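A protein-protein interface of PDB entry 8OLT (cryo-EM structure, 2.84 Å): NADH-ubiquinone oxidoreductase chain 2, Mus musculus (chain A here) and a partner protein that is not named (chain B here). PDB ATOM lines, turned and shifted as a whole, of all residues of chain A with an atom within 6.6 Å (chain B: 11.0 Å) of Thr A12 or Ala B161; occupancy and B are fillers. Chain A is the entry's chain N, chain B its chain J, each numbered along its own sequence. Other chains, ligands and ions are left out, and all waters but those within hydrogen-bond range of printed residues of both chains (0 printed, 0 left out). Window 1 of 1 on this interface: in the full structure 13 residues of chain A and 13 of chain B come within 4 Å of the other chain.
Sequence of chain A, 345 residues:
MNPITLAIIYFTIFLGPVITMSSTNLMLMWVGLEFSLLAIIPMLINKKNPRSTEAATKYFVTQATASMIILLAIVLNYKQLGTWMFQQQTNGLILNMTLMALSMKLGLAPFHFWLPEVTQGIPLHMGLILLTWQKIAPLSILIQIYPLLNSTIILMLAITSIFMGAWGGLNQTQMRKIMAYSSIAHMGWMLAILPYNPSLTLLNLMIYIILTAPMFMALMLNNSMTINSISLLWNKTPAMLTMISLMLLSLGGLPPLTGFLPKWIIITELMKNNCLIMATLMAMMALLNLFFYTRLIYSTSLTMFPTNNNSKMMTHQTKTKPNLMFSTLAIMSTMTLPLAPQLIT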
ATOM      1  N   LEU A   6     -20.892  13.081 -24.165  1.00  0.00           N
ATOM      2  CA  LEU A   6     -21.544  11.778 -24.126  1.00  0.00           C
ATOM      3  C   LEU A   6     -20.573  10.695 -23.691  1.00  0.00           C
ATOM      4  O   LEU A   6     -20.887   9.874 -22.828  1.00  0.00           O
ATOM      5  CB  LEU A   6     -22.130  11.442 -25.493  1.00  0.00           C
ATOM      6  CG  LEU A   6     -23.275  12.327 -25.972  1.00  0.00           C
ATOM      7  CD1 LEU A   6     -23.401  12.220 -27.467  1.00  0.00           C
ATOM      8  CD2 LEU A   6     -24.565  11.936 -25.319  1.00  0.00           C
ATOM      9  N   ALA A   7     -19.378  10.684 -24.271  1.00  0.00           N
ATOM     10  CA  ALA A   7     -18.392   9.691 -23.878  1.00  0.00           C
ATOM     11  C   ALA A   7     -18.084   9.788 -22.393  1.00  0.00           C
ATOM     12  O   ALA A   7     -17.979   8.770 -21.705  1.00  0.00           O
ATOM     13  CB  ALA A   7     -17.118   9.865 -24.697  1.00  0.00           C
ATOM     14  N   ILE A   8     -17.929  11.004 -21.880  1.00  0.00           N
ATOM     15  CA  ILE A   8     -17.620  11.171 -20.467  1.00  0.00           C
ATOM     16  C   ILE A   8     -18.825  10.810 -19.615  1.00  0.00           C
ATOM     17  O   ILE A   8     -18.704  10.114 -18.604  1.00  0.00           O
ATOM     18  CB  ILE A   8     -17.146  12.610 -20.194  1.00  0.00           C
ATOM     19  CG1 ILE A   8     -15.807  12.864 -20.876  1.00  0.00           C
ATOM     20  CG2 ILE A   8     -17.039  12.875 -18.702  1.00  0.00           C
ATOM     21  CD1 ILE A   8     -14.665  12.180 -20.222  1.00  0.00           C
ATOM     22  N   ILE A   9     -20.004  11.284 -19.997  1.00  0.00           N
ATOM     23  CA  ILE A   9     -21.181  11.072 -19.166  1.00  0.00           C
ATOM     24  C   ILE A   9     -21.667   9.633 -19.260  1.00  0.00           C
ATOM     25  O   ILE A   9     -22.001   9.019 -18.245  1.00  0.00           O
ATOM     26  CB  ILE A   9     -22.276  12.083 -19.544  1.00  0.00           C
ATOM     27  CG1 ILE A   9     -21.834  13.483 -19.111  1.00  0.00           C
ATOM     28  CG2 ILE A   9     -23.592  11.701 -18.902  1.00  0.00           C
ATOM     29  CD1 ILE A   9     -22.836  14.586 -19.354  1.00  0.00           C
ATOM     30  N   TYR A  10     -21.705   9.056 -20.460  1.00  0.00           N
ATOM     31  CA  TYR A  10     -22.170   7.676 -20.565  1.00  0.00           C
ATOM     32  C   TYR A  10     -21.175   6.698 -19.973  1.00  0.00           C
ATOM     33  O   TYR A  10     -21.578   5.659 -19.445  1.00  0.00           O
ATOM     34  CB  TYR A  10     -22.462   7.303 -22.012  1.00  0.00           C
ATOM     35  CG  TYR A  10     -23.850   7.683 -22.437  1.00  0.00           C
ATOM     36  CD1 TYR A  10     -24.054   8.552 -23.482  1.00  0.00           C
ATOM     37  CD2 TYR A  10     -24.957   7.178 -21.783  1.00  0.00           C
ATOM     38  CE1 TYR A  10     -25.314   8.912 -23.868  1.00  0.00           C
ATOM     39  CE2 TYR A  10     -26.229   7.534 -22.165  1.00  0.00           C
ATOM     40  CZ  TYR A  10     -26.398   8.400 -23.211  1.00  0.00           C
ATOM     41  OH  TYR A  10     -27.659   8.767 -23.612  1.00  0.00           O
ATOM     42  N   PHE A  11     -19.884   6.994 -20.055  1.00  0.00           N
ATOM     43  CA  PHE A  11     -18.906   6.142 -19.396  1.00  0.00           C
ATOM     44  C   PHE A  11     -19.088   6.182 -17.888  1.00  0.00           C
ATOM     45  O   PHE A  11     -19.055   5.147 -17.223  1.00  0.00           O
ATOM     46  CB  PHE A  11     -17.504   6.577 -19.790  1.00  0.00           C
ATOM     47  CG  PHE A  11     -16.425   5.795 -19.129  1.00  0.00           C
ATOM     48  CD1 PHE A  11     -16.168   4.497 -19.501  1.00  0.00           C
ATOM     49  CD2 PHE A  11     -15.652   6.366 -18.143  1.00  0.00           C
ATOM     50  CE1 PHE A  11     -15.173   3.780 -18.898  1.00  0.00           C
ATOM     51  CE2 PHE A  11     -14.652   5.653 -17.541  1.00  0.00           C
ATOM     52  CZ  PHE A  11     -14.411   4.359 -17.919  1.00  0.00           C
ATOM     53  N   THR A  12     -19.322   7.367 -17.333  1.00  0.00           N
ATOM     54  CA  THR A  12     -19.503   7.484 -15.895  1.00  0.00           C
ATOM     55  C   THR A  12     -20.761   6.764 -15.429  1.00  0.00           C
ATOM     56  O   THR A  12     -20.771   6.159 -14.353  1.00  0.00           O
ATOM     57  CB  THR A  12     -19.549   8.954 -15.505  1.00  0.00           C
ATOM     58  OG1 THR A  12     -18.324   9.579 -15.885  1.00  0.00           O
ATOM     59  CG2 THR A  12     -19.729   9.103 -14.016  1.00  0.00           C
ATOM     60  N   ILE A  13     -21.840   6.837 -16.210  1.00  0.00           N
ATOM     61  CA  ILE A  13     -23.057   6.113 -15.861  1.00  0.00           C
ATOM     62  C   ILE A  13     -22.782   4.624 -15.818  1.00  0.00           C
ATOM     63  O   ILE A  13     -23.244   3.912 -14.925  1.00  0.00           O
ATOM     64  CB  ILE A  13     -24.181   6.438 -16.858  1.00  0.00           C
ATOM     65  CG1 ILE A  13     -24.678   7.855 -16.645  1.00  0.00           C
ATOM     66  CG2 ILE A  13     -25.329   5.491 -16.681  1.00  0.00           C
ATOM     67  CD1 ILE A  13     -25.391   8.424 -17.833  1.00  0.00           C
ATOM     68  N   PHE A  14     -22.044   4.128 -16.796  1.00  0.00           N
ATOM     69  CA  PHE A  14     -21.657   2.729 -16.788  1.00  0.00           C
ATOM     70  C   PHE A  14     -20.669   2.443 -15.669  1.00  0.00           C
ATOM     71  O   PHE A  14     -20.717   1.378 -15.046  1.00  0.00           O
ATOM     72  CB  PHE A  14     -21.078   2.375 -18.154  1.00  0.00           C
ATOM     73  CG  PHE A  14     -20.323   1.096 -18.180  1.00  0.00           C
ATOM     74  CD1 PHE A  14     -20.984  -0.110 -18.160  1.00  0.00           C
ATOM     75  CD2 PHE A  14     -18.948   1.099 -18.242  1.00  0.00           C
ATOM     76  CE1 PHE A  14     -20.288  -1.286 -18.188  1.00  0.00           C
ATOM     77  CE2 PHE A  14     -18.248  -0.077 -18.275  1.00  0.00           C
ATOM     78  CZ  PHE A  14     -18.919  -1.271 -18.247  1.00  0.00           C
ATOM     79  N   LEU A  15     -19.779   3.388 -15.385  1.00  0.00           N
ATOM     80  CA  LEU A  15     -18.709   3.132 -14.432  1.00  0.00           C
ATOM     81  C   LEU A  15     -19.241   2.911 -13.024  1.00  0.00           C
ATOM     82  O   LEU A  15     -18.767   2.021 -12.315  1.00  0.00           O
ATOM     83  CB  LEU A  15     -17.722   4.293 -14.444  1.00  0.00           C
ATOM     84  CG  LEU A  15     -16.424   4.019 -13.705  1.00  0.00           C
ATOM     85  CD1 LEU A  15     -15.553   3.088 -14.509  1.00  0.00           C
ATOM     86  CD2 LEU A  15     -15.716   5.313 -13.409  1.00  0.00           C
ATOM     87  N   GLY A  16     -20.216   3.708 -12.604  1.00  0.00           N
ATOM     88  CA  GLY A  16     -20.732   3.660 -11.259  1.00  0.00           C
ATOM     89  C   GLY A  16     -21.067   2.267 -10.771  1.00  0.00           C
ATOM     90  O   GLY A  16     -20.464   1.759  -9.822  1.00  0.00           O
ATOM     91  N   PRO A  17     -22.052   1.624 -11.395  1.00  0.00           N
ATOM     92  CA  PRO A  17     -22.419   0.277 -10.955  1.00  0.00           C
ATOM     93  C   PRO A  17     -21.276  -0.712 -11.010  1.00  0.00           C
ATOM     94  O   PRO A  17     -21.205  -1.603 -10.159  1.00  0.00           O
ATOM     95  CB  PRO A  17     -23.546  -0.095 -11.918  1.00  0.00           C
ATOM     96  CG  PRO A  17     -24.177   1.183 -12.210  1.00  0.00           C
ATOM     97  CD  PRO A  17     -23.048   2.167 -12.327  1.00  0.00           C
ATOM     98  N   GLY A  32     -19.364   4.432  -6.027  1.00  0.00           N
ATOM     99  CA  GLY A  32     -20.085   4.059  -7.226  1.00  0.00           C
ATOM    100  C   GLY A  32     -21.521   4.541  -7.220  1.00  0.00           C
ATOM    101  O   GLY A  32     -22.075   4.874  -8.264  1.00  0.00           O
ATOM    102  N   GLU A  34     -22.405   7.303  -5.976  1.00  0.00           N
ATOM    103  CA  GLU A  34     -22.318   8.728  -6.268  1.00  0.00           C
ATOM    104  C   GLU A  34     -22.117   8.970  -7.751  1.00  0.00           C
ATOM    105  O   GLU A  34     -22.704   9.894  -8.316  1.00  0.00           O
ATOM    106  CB  GLU A  34     -21.174   9.359  -5.483  1.00  0.00           C
ATOM    107  CG  GLU A  34     -21.263   9.150  -4.014  1.00  0.00           C
ATOM    108  CD  GLU A  34     -22.565   9.633  -3.468  1.00  0.00           C
ATOM    109  OE1 GLU A  34     -23.068  10.647  -3.978  1.00  0.00           O
ATOM    110  OE2 GLU A  34     -23.094   9.002  -2.538  1.00  0.00           O
ATOM    111  N   PHE A  35     -21.291   8.152  -8.397  1.00  0.00           N
ATOM    112  CA  PHE A  35     -21.070   8.313  -9.827  1.00  0.00           C
ATOM    113  C   PHE A  35     -22.375   8.191 -10.591  1.00  0.00           C
ATOM    114  O   PHE A  35     -22.643   8.977 -11.505  1.00  0.00           O
ATOM    115  CB  PHE A  35     -20.073   7.271 -10.335  1.00  0.00           C
ATOM    116  CG  PHE A  35     -18.633   7.626 -10.113  1.00  0.00           C
ATOM    117  CD1 PHE A  35     -18.184   8.922 -10.243  1.00  0.00           C
ATOM    118  CD2 PHE A  35     -17.724   6.651  -9.784  1.00  0.00           C
ATOM    119  CE1 PHE A  35     -16.865   9.229 -10.047  1.00  0.00           C
ATOM    120  CE2 PHE A  35     -16.397   6.958  -9.587  1.00  0.00           C
ATOM    121  CZ  PHE A  35     -15.970   8.245  -9.716  1.00  0.00           C
ATOM    122  N   SER A  36     -23.196   7.203 -10.243  1.00  0.00           N
ATOM    123  CA  SER A  36     -24.468   7.041 -10.930  1.00  0.00           C
ATOM    124  C   SER A  36     -25.376   8.232 -10.686  1.00  0.00           C
ATOM    125  O   SER A  36     -26.030   8.719 -11.609  1.00  0.00           O
ATOM    126  CB  SER A  36     -25.151   5.755 -10.476  1.00  0.00           C
ATOM    127  OG  SER A  36     -24.285   4.650 -10.588  1.00  0.00           O
ATOM    128  N   LEU A  38     -24.603  11.363  -9.934  1.00  0.00           N
ATOM    129  CA  LEU A  38     -24.145  12.601 -10.544  1.00  0.00           C
ATOM    130  C   LEU A  38     -24.308  12.569 -12.054  1.00  0.00           C
ATOM    131  O   LEU A  38     -24.795  13.531 -12.655  1.00  0.00           O
ATOM    132  CB  LEU A  38     -22.691  12.856 -10.167  1.00  0.00           C
ATOM    133  CG  LEU A  38     -22.450  12.982  -8.665  1.00  0.00           C
ATOM    134  CD1 LEU A  38     -20.977  13.135  -8.367  1.00  0.00           C
ATOM    135  CD2 LEU A  38     -23.243  14.134  -8.088  1.00  0.00           C
ATOM    136  N   ALA A  39     -23.899  11.476 -12.689  1.00  0.00           N
ATOM    137  CA  ALA A  39     -23.847  11.451 -14.144  1.00  0.00           C
ATOM    138  C   ALA A  39     -25.219  11.291 -14.781  1.00  0.00           C
ATOM    139  O   ALA A  39     -25.408  11.703 -15.925  1.00  0.00           O
ATOM    140  CB  ALA A  39     -22.930  10.336 -14.621  1.00  0.00           C
ATOM    141  N   MET B 152      -7.550   7.905  -5.378  1.00  0.00           N
ATOM    142  CA  MET B 152      -7.321   9.118  -6.142  1.00  0.00           C
ATOM    143  C   MET B 152      -7.871   9.024  -7.553  1.00  0.00           C
ATOM    144  O   MET B 152      -8.302  10.035  -8.106  1.00  0.00           O
ATOM    145  CB  MET B 152      -5.830   9.413  -6.185  1.00  0.00           C
ATOM    146  CG  MET B 152      -5.493  10.782  -6.722  1.00  0.00           C
ATOM    147  SD  MET B 152      -3.726  11.058  -6.762  1.00  0.00           S
ATOM    148  CE  MET B 152      -3.388  11.117  -5.021  1.00  0.00           C
ATOM    149  N   VAL B 153      -7.869   7.837  -8.153  1.00  0.00           N
ATOM    150  CA  VAL B 153      -8.449   7.688  -9.484  1.00  0.00           C
ATOM    151  C   VAL B 153      -9.926   8.050  -9.455  1.00  0.00           C
ATOM    152  O   VAL B 153     -10.405   8.839 -10.273  1.00  0.00           O
ATOM    153  CB  VAL B 153      -8.227   6.260 -10.009  1.00  0.00           C
ATOM    154  CG1 VAL B 153      -9.003   6.039 -11.282  1.00  0.00           C
ATOM    155  CG2 VAL B 153      -6.767   6.008 -10.249  1.00  0.00           C
ATOM    156  N   VAL B 154     -10.669   7.490  -8.504  1.00  0.00           N
ATOM    157  CA  VAL B 154     -12.096   7.775  -8.432  1.00  0.00           C
ATOM    158  C   VAL B 154     -12.330   9.222  -8.024  1.00  0.00           C
ATOM    159  O   VAL B 154     -13.289   9.856  -8.469  1.00  0.00           O
ATOM    160  CB  VAL B 154     -12.799   6.794  -7.476  1.00  0.00           C
ATOM    161  CG1 VAL B 154     -12.491   5.378  -7.859  1.00  0.00           C
ATOM    162  CG2 VAL B 154     -12.403   7.054  -6.043  1.00  0.00           C
ATOM    163  N   ALA B 155     -11.481   9.759  -7.157  1.00  0.00           N
ATOM    164  CA  ALA B 155     -11.631  11.148  -6.750  1.00  0.00           C
ATOM    165  C   ALA B 155     -11.328  12.085  -7.906  1.00  0.00           C
ATOM    166  O   ALA B 155     -12.108  12.994  -8.203  1.00  0.00           O
ATOM    167  CB  ALA B 155     -10.726  11.445  -5.561  1.00  0.00           C
ATOM    168  N   GLY B 156     -10.209  11.864  -8.586  1.00  0.00           N
ATOM    169  CA  GLY B 156      -9.898  12.672  -9.747  1.00  0.00           C
ATOM    170  C   GLY B 156     -10.948  12.557 -10.833  1.00  0.00           C
ATOM    171  O   GLY B 156     -11.326  13.554 -11.445  1.00  0.00           O
ATOM    172  N   TRP B 157     -11.419  11.339 -11.103  1.00  0.00           N
ATOM    173  CA  TRP B 157     -12.439  11.173 -12.130  1.00  0.00           C
ATOM    174  C   TRP B 157     -13.741  11.839 -11.722  1.00  0.00           C
ATOM    175  O   TRP B 157     -14.431  12.427 -12.556  1.00  0.00           O
ATOM    176  CB  TRP B 157     -12.684   9.700 -12.433  1.00  0.00           C
ATOM    177  CG  TRP B 157     -13.648   9.568 -13.547  1.00  0.00           C
ATOM    178  CD1 TRP B 157     -14.992   9.408 -13.450  1.00  0.00           C
ATOM    179  CD2 TRP B 157     -13.352   9.636 -14.939  1.00  0.00           C
ATOM    180  NE1 TRP B 157     -15.552   9.358 -14.693  1.00  0.00           N
ATOM    181  CE2 TRP B 157     -14.564   9.495 -15.628  1.00  0.00           C
ATOM    182  CE3 TRP B 157     -12.175   9.791 -15.673  1.00  0.00           C
ATOM    183  CZ2 TRP B 157     -14.637   9.506 -17.010  1.00  0.00           C
ATOM    184  CZ3 TRP B 157     -12.250   9.796 -17.039  1.00  0.00           C
ATOM    185  CH2 TRP B 157     -13.470   9.654 -17.698  1.00  0.00           C
ATOM    186  N   SER B 158     -14.095  11.756 -10.444  1.00  0.00           N
ATOM    187  CA  SER B 158     -15.294  12.424  -9.961  1.00  0.00           C
ATOM    188  C   SER B 158     -15.264  13.903 -10.298  1.00  0.00           C
ATOM    189  O   SER B 158     -16.248  14.464 -10.787  1.00  0.00           O
ATOM    190  CB  SER B 158     -15.412  12.222  -8.456  1.00  0.00           C
ATOM    191  OG  SER B 158     -16.639  12.722  -7.969  1.00  0.00           O
ATOM    192  N   LEU B 159     -14.137  14.556 -10.039  1.00  0.00           N
ATOM    193  CA  LEU B 159     -14.037  15.984 -10.300  1.00  0.00           C
ATOM    194  C   LEU B 159     -13.944  16.262 -11.788  1.00  0.00           C
ATOM    195  O   LEU B 159     -14.552  17.212 -12.286  1.00  0.00           O
ATOM    196  CB  LEU B 159     -12.827  16.552  -9.569  1.00  0.00           C
ATOM    197  CG  LEU B 159     -12.857  16.297  -8.064  1.00  0.00           C
ATOM    198  CD1 LEU B 159     -11.466  16.306  -7.488  1.00  0.00           C
ATOM    199  CD2 LEU B 159     -13.723  17.324  -7.367  1.00  0.00           C
ATOM    200  N   PHE B 160     -13.197  15.434 -12.515  1.00  0.00           N
ATOM    201  CA  PHE B 160     -13.069  15.606 -13.955  1.00  0.00           C
ATOM    202  C   PHE B 160     -14.426  15.520 -14.632  1.00  0.00           C
ATOM    203  O   PHE B 160     -14.804  16.399 -15.409  1.00  0.00           O
ATOM    204  CB  PHE B 160     -12.115  14.551 -14.508  1.00  0.00           C
ATOM    205  CG  PHE B 160     -11.908  14.636 -15.986  1.00  0.00           C
ATOM    206  CD1 PHE B 160     -11.257  15.714 -16.543  1.00  0.00           C
ATOM    207  CD2 PHE B 160     -12.346  13.631 -16.814  1.00  0.00           C
ATOM    208  CE1 PHE B 160     -11.068  15.795 -17.890  1.00  0.00           C
ATOM    209  CE2 PHE B 160     -12.156  13.715 -18.164  1.00  0.00           C
ATOM    210  CZ  PHE B 160     -11.514  14.800 -18.701  1.00  0.00           C
ATOM    211  N   ALA B 161     -15.183  14.470 -14.331  1.00  0.00           N
ATOM    212  CA  ALA B 161     -16.510  14.332 -14.904  1.00  0.00           C
ATOM    213  C   ALA B 161     -17.418  15.475 -14.486  1.00  0.00           C
ATOM    214  O   ALA B 161     -18.253  15.920 -15.275  1.00  0.00           O
ATOM    215  CB  ALA B 161     -17.114  12.995 -14.490  1.00  0.00           C
ATOM    216  N   GLY B 162     -17.267  15.968 -13.258  1.00  0.00           N
ATOM    217  CA  GLY B 162     -18.161  17.000 -12.768  1.00  0.00           C
ATOM    218  C   GLY B 162     -18.133  18.257 -13.612  1.00  0.00           C
ATOM    219  O   GLY B 162     -19.161  18.908 -13.802  1.00  0.00           O
ATOM    220  N   ILE B 163     -16.960  18.622 -14.124  1.00  0.00           N
ATOM    221  CA  ILE B 163     -16.872  19.788 -14.992  1.00  0.00           C
ATOM    222  C   ILE B 163     -17.737  19.591 -16.221  1.00  0.00           C
ATOM    223  O   ILE B 163     -18.447  20.506 -16.654  1.00  0.00           O
ATOM    224  CB  ILE B 163     -15.410  20.059 -15.385  1.00  0.00           C
ATOM    225  CG1 ILE B 163     -14.604  20.500 -14.176  1.00  0.00           C
ATOM    226  CG2 ILE B 163     -15.344  21.120 -16.453  1.00  0.00           C
ATOM    227  CD1 ILE B 163     -13.144  20.180 -14.297  1.00  0.00           C
ATOM    228  N   PHE B 164     -17.669  18.410 -16.822  1.00  0.00           N
ATOM    229  CA  PHE B 164     -18.540  18.110 -17.944  1.00  0.00           C
ATOM    230  C   PHE B 164     -19.995  18.061 -17.513  1.00  0.00           C
ATOM    231  O   PHE B 164     -20.879  18.439 -18.282  1.00  0.00           O
ATOM    232  CB  PHE B 164     -18.126  16.789 -18.576  1.00  0.00           C
ATOM    233  CG  PHE B 164     -16.785  16.831 -19.238  1.00  0.00           C
ATOM    234  CD1 PHE B 164     -15.627  16.756 -18.495  1.00  0.00           C
ATOM    235  CD2 PHE B 164     -16.687  16.930 -20.604  1.00  0.00           C
ATOM    236  CE1 PHE B 164     -14.405  16.787 -19.108  1.00  0.00           C
ATOM    237  CE2 PHE B 164     -15.471  16.959 -21.211  1.00  0.00           C
ATOM    238  CZ  PHE B 164     -14.326  16.894 -20.466  1.00  0.00           C
ATOM    239  N   ILE B 165     -20.254  17.599 -16.293  1.00  0.00           N
ATOM    240  CA  ILE B 165     -21.623  17.439 -15.820  1.00  0.00           C
ATOM    241  C   ILE B 165     -22.287  18.793 -15.625  1.00  0.00           C
ATOM    242  O   ILE B 165     -23.432  19.002 -16.038  1.00  0.00           O
ATOM    243  CB  ILE B 165     -21.638  16.613 -14.525  1.00  0.00           C
ATOM    244  CG1 ILE B 165     -21.318  15.156 -14.846  1.00  0.00           C
ATOM    245  CG2 ILE B 165     -22.975  16.747 -13.825  1.00  0.00           C
ATOM    246  CD1 ILE B 165     -21.077  14.301 -13.632  1.00  0.00           C
ATOM    247  N   ILE B 166     -21.591  19.730 -14.984  1.00  0.00           N
ATOM    248  CA  ILE B 166     -22.209  21.019 -14.688  1.00  0.00           C
ATOM    249  C   ILE B 166     -22.326  21.864 -15.946  1.00  0.00           C
ATOM    250  O   ILE B 166     -23.286  22.623 -16.104  1.00  0.00           O
ATOM    251  CB  ILE B 166     -21.437  21.764 -13.586  1.00  0.00           C
ATOM    252  CG1 ILE B 166     -19.991  22.025 -14.014  1.00  0.00           C
ATOM    253  CG2 ILE B 166     -21.485  20.977 -12.299  1.00  0.00           C
ATOM    254  CD1 ILE B 166     -19.213  22.868 -13.036  1.00  0.00           C
ATOM    255  N   ILE B 167     -21.356  21.773 -16.851  1.00  0.00           N
ATOM    256  CA  ILE B 167     -21.425  22.605 -18.046  1.00  0.00           C
ATOM    257  C   ILE B 167     -22.656  22.241 -18.860  1.00  0.00           C
ATOM    258  O   ILE B 167     -23.277  23.102 -19.491  1.00  0.00           O
ATOM    259  CB  ILE B 167     -20.129  22.489 -18.867  1.00  0.00           C
ATOM    260  CG1 ILE B 167     -19.018  23.287 -18.187  1.00  0.00           C
ATOM    261  CG2 ILE B 167     -20.342  23.007 -20.262  1.00  0.00           C
ATOM    262  CD1 ILE B 167     -17.656  23.022 -18.740  1.00  0.00           C
ATOM    263  N   GLU B 168     -23.032  20.963 -18.857  1.00  0.00           N
ATOM    264  CA  GLU B 168     -24.246  20.545 -19.540  1.00  0.00           C
ATOM    265  C   GLU B 168     -25.504  20.874 -18.754  1.00  0.00           C
ATOM    266  O   GLU B 168     -26.530  21.186 -19.360  1.00  0.00           O
ATOM    267  CB  GLU B 168     -24.209  19.048 -19.824  1.00  0.00           C
ATOM    268  CG  GLU B 168     -23.614  18.695 -21.155  1.00  0.00           C
ATOM    269  CD  GLU B 168     -24.296  19.395 -22.317  1.00  0.00           C
ATOM    270  OE1 GLU B 168     -23.631  20.204 -22.989  1.00  0.00           O
ATOM    271  OE2 GLU B 168     -25.496  19.149 -22.556  1.00  0.00           O
ATOM    272  N   ILE B 169     -25.461  20.794 -17.425  1.00  0.00           N
ATOM    273  CA  ILE B 169     -26.656  21.083 -16.640  1.00  0.00           C
ATOM    274  C   ILE B 169     -27.054  22.538 -16.799  1.00  0.00           C
ATOM    275  O   ILE B 169     -28.236  22.858 -16.954  1.00  0.00           O
ATOM    276  CB  ILE B 169     -26.442  20.737 -15.158  1.00  0.00           C
ATOM    277  CG1 ILE B 169     -26.417  19.232 -14.958  1.00  0.00           C
ATOM    278  CG2 ILE B 169     -27.566  21.327 -14.322  1.00  0.00           C
ATOM    279  CD1 ILE B 169     -26.064  18.807 -13.555  1.00  0.00           C
ATOM    280  N   THR B 170     -26.084  23.440 -16.730  1.00  0.00           N
ATOM    281  CA  THR B 170     -26.351  24.866 -16.773  1.00  0.00           C
ATOM    282  C   THR B 170     -26.485  25.401 -18.188  1.00  0.00           C
ATOM    283  O   THR B 170     -26.996  26.510 -18.362  1.00  0.00           O
ATOM    284  CB  THR B 170     -25.236  25.615 -16.048  1.00  0.00           C
ATOM    285  OG1 THR B 170     -23.969  25.106 -16.472  1.00  0.00           O
ATOM    286  CG2 THR B 170     -25.369  25.431 -14.561  1.00  0.00           C
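The indole nitrogen (NE1) of Trp B157 lies within hydrogen-bond range of the side-chain hydroxyl (OG1) of Thr A12, at 3.0 Å.
OG1 of Thr A12 lies within hydrogen-bond range of O of Ile A8, at 2.8 Å.
Ile A8 touches Trp B157 (CD1 to CH2, 3.8 Å). CD1 of Ile A8 touches CE2 of Phe B160 (3.6 Å). Trp B157 touches Phe A11. Thr A12 touches Ala B161 (OG1 to CB, 3.9 Å). Phe A35 touches Val B154 (CZ to O, 3.4 Å). Trp B157 touches Phe A35 (CD1 to CE1, 3.9 Å). Phe A35 touches Ser B158 (CE1 to CA, 3.6 Å). O of Leu A38 touches CG2 of Ile B165, at 3.9 Å.
Of the printed residues of chain A, Ala B161 touches Thr A12 (3.9 Å). No residue of chain B comes within 4 Å of Ile A9. Phe A11 touches just one residue of chain B: Trp B157 (3.5 Å). Ile A13 touches none of the printed residues of chain B. No residue of chain B comes within 4 Å of Leu A15. Gly A16 touches none of the printed residues of chain B. Phe A35 touches just these residues of chain B: Val B154 (3.4 Å), Trp B157 (3.9 Å) and Ser B158 (3.6 Å). No residue of chain B comes within 4 Å of Ser A36. Printed residues of chain A within 4 Å of Trp B157: Ile A8, Phe A11, Thr A12 and Phe A35. Of the printed residues of chain B, Leu A38 touches Ile B165 (3.9 Å). Printed residues of chain A within 4 Å of Val B154: Phe A35. Printed residues of chain A within 4 Å of Ser B158: Phe A35. Printed residues of chain B within 4 Å of Ile A8: Trp B157 (3.8 Å) and Phe B160 (3.6 Å). Ala A39 touches none of the printed residues of chain B.
Printed residues of chain B that touch a printed residue of chain A: Val B154, Trp B157, Ser B158, Phe B160, Ala B161 and Ile B165. Of the 18 printed residues of chain A, 5 touch a printed residue of chain B. Among the printed residues, 9 pairs touch across the chains.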
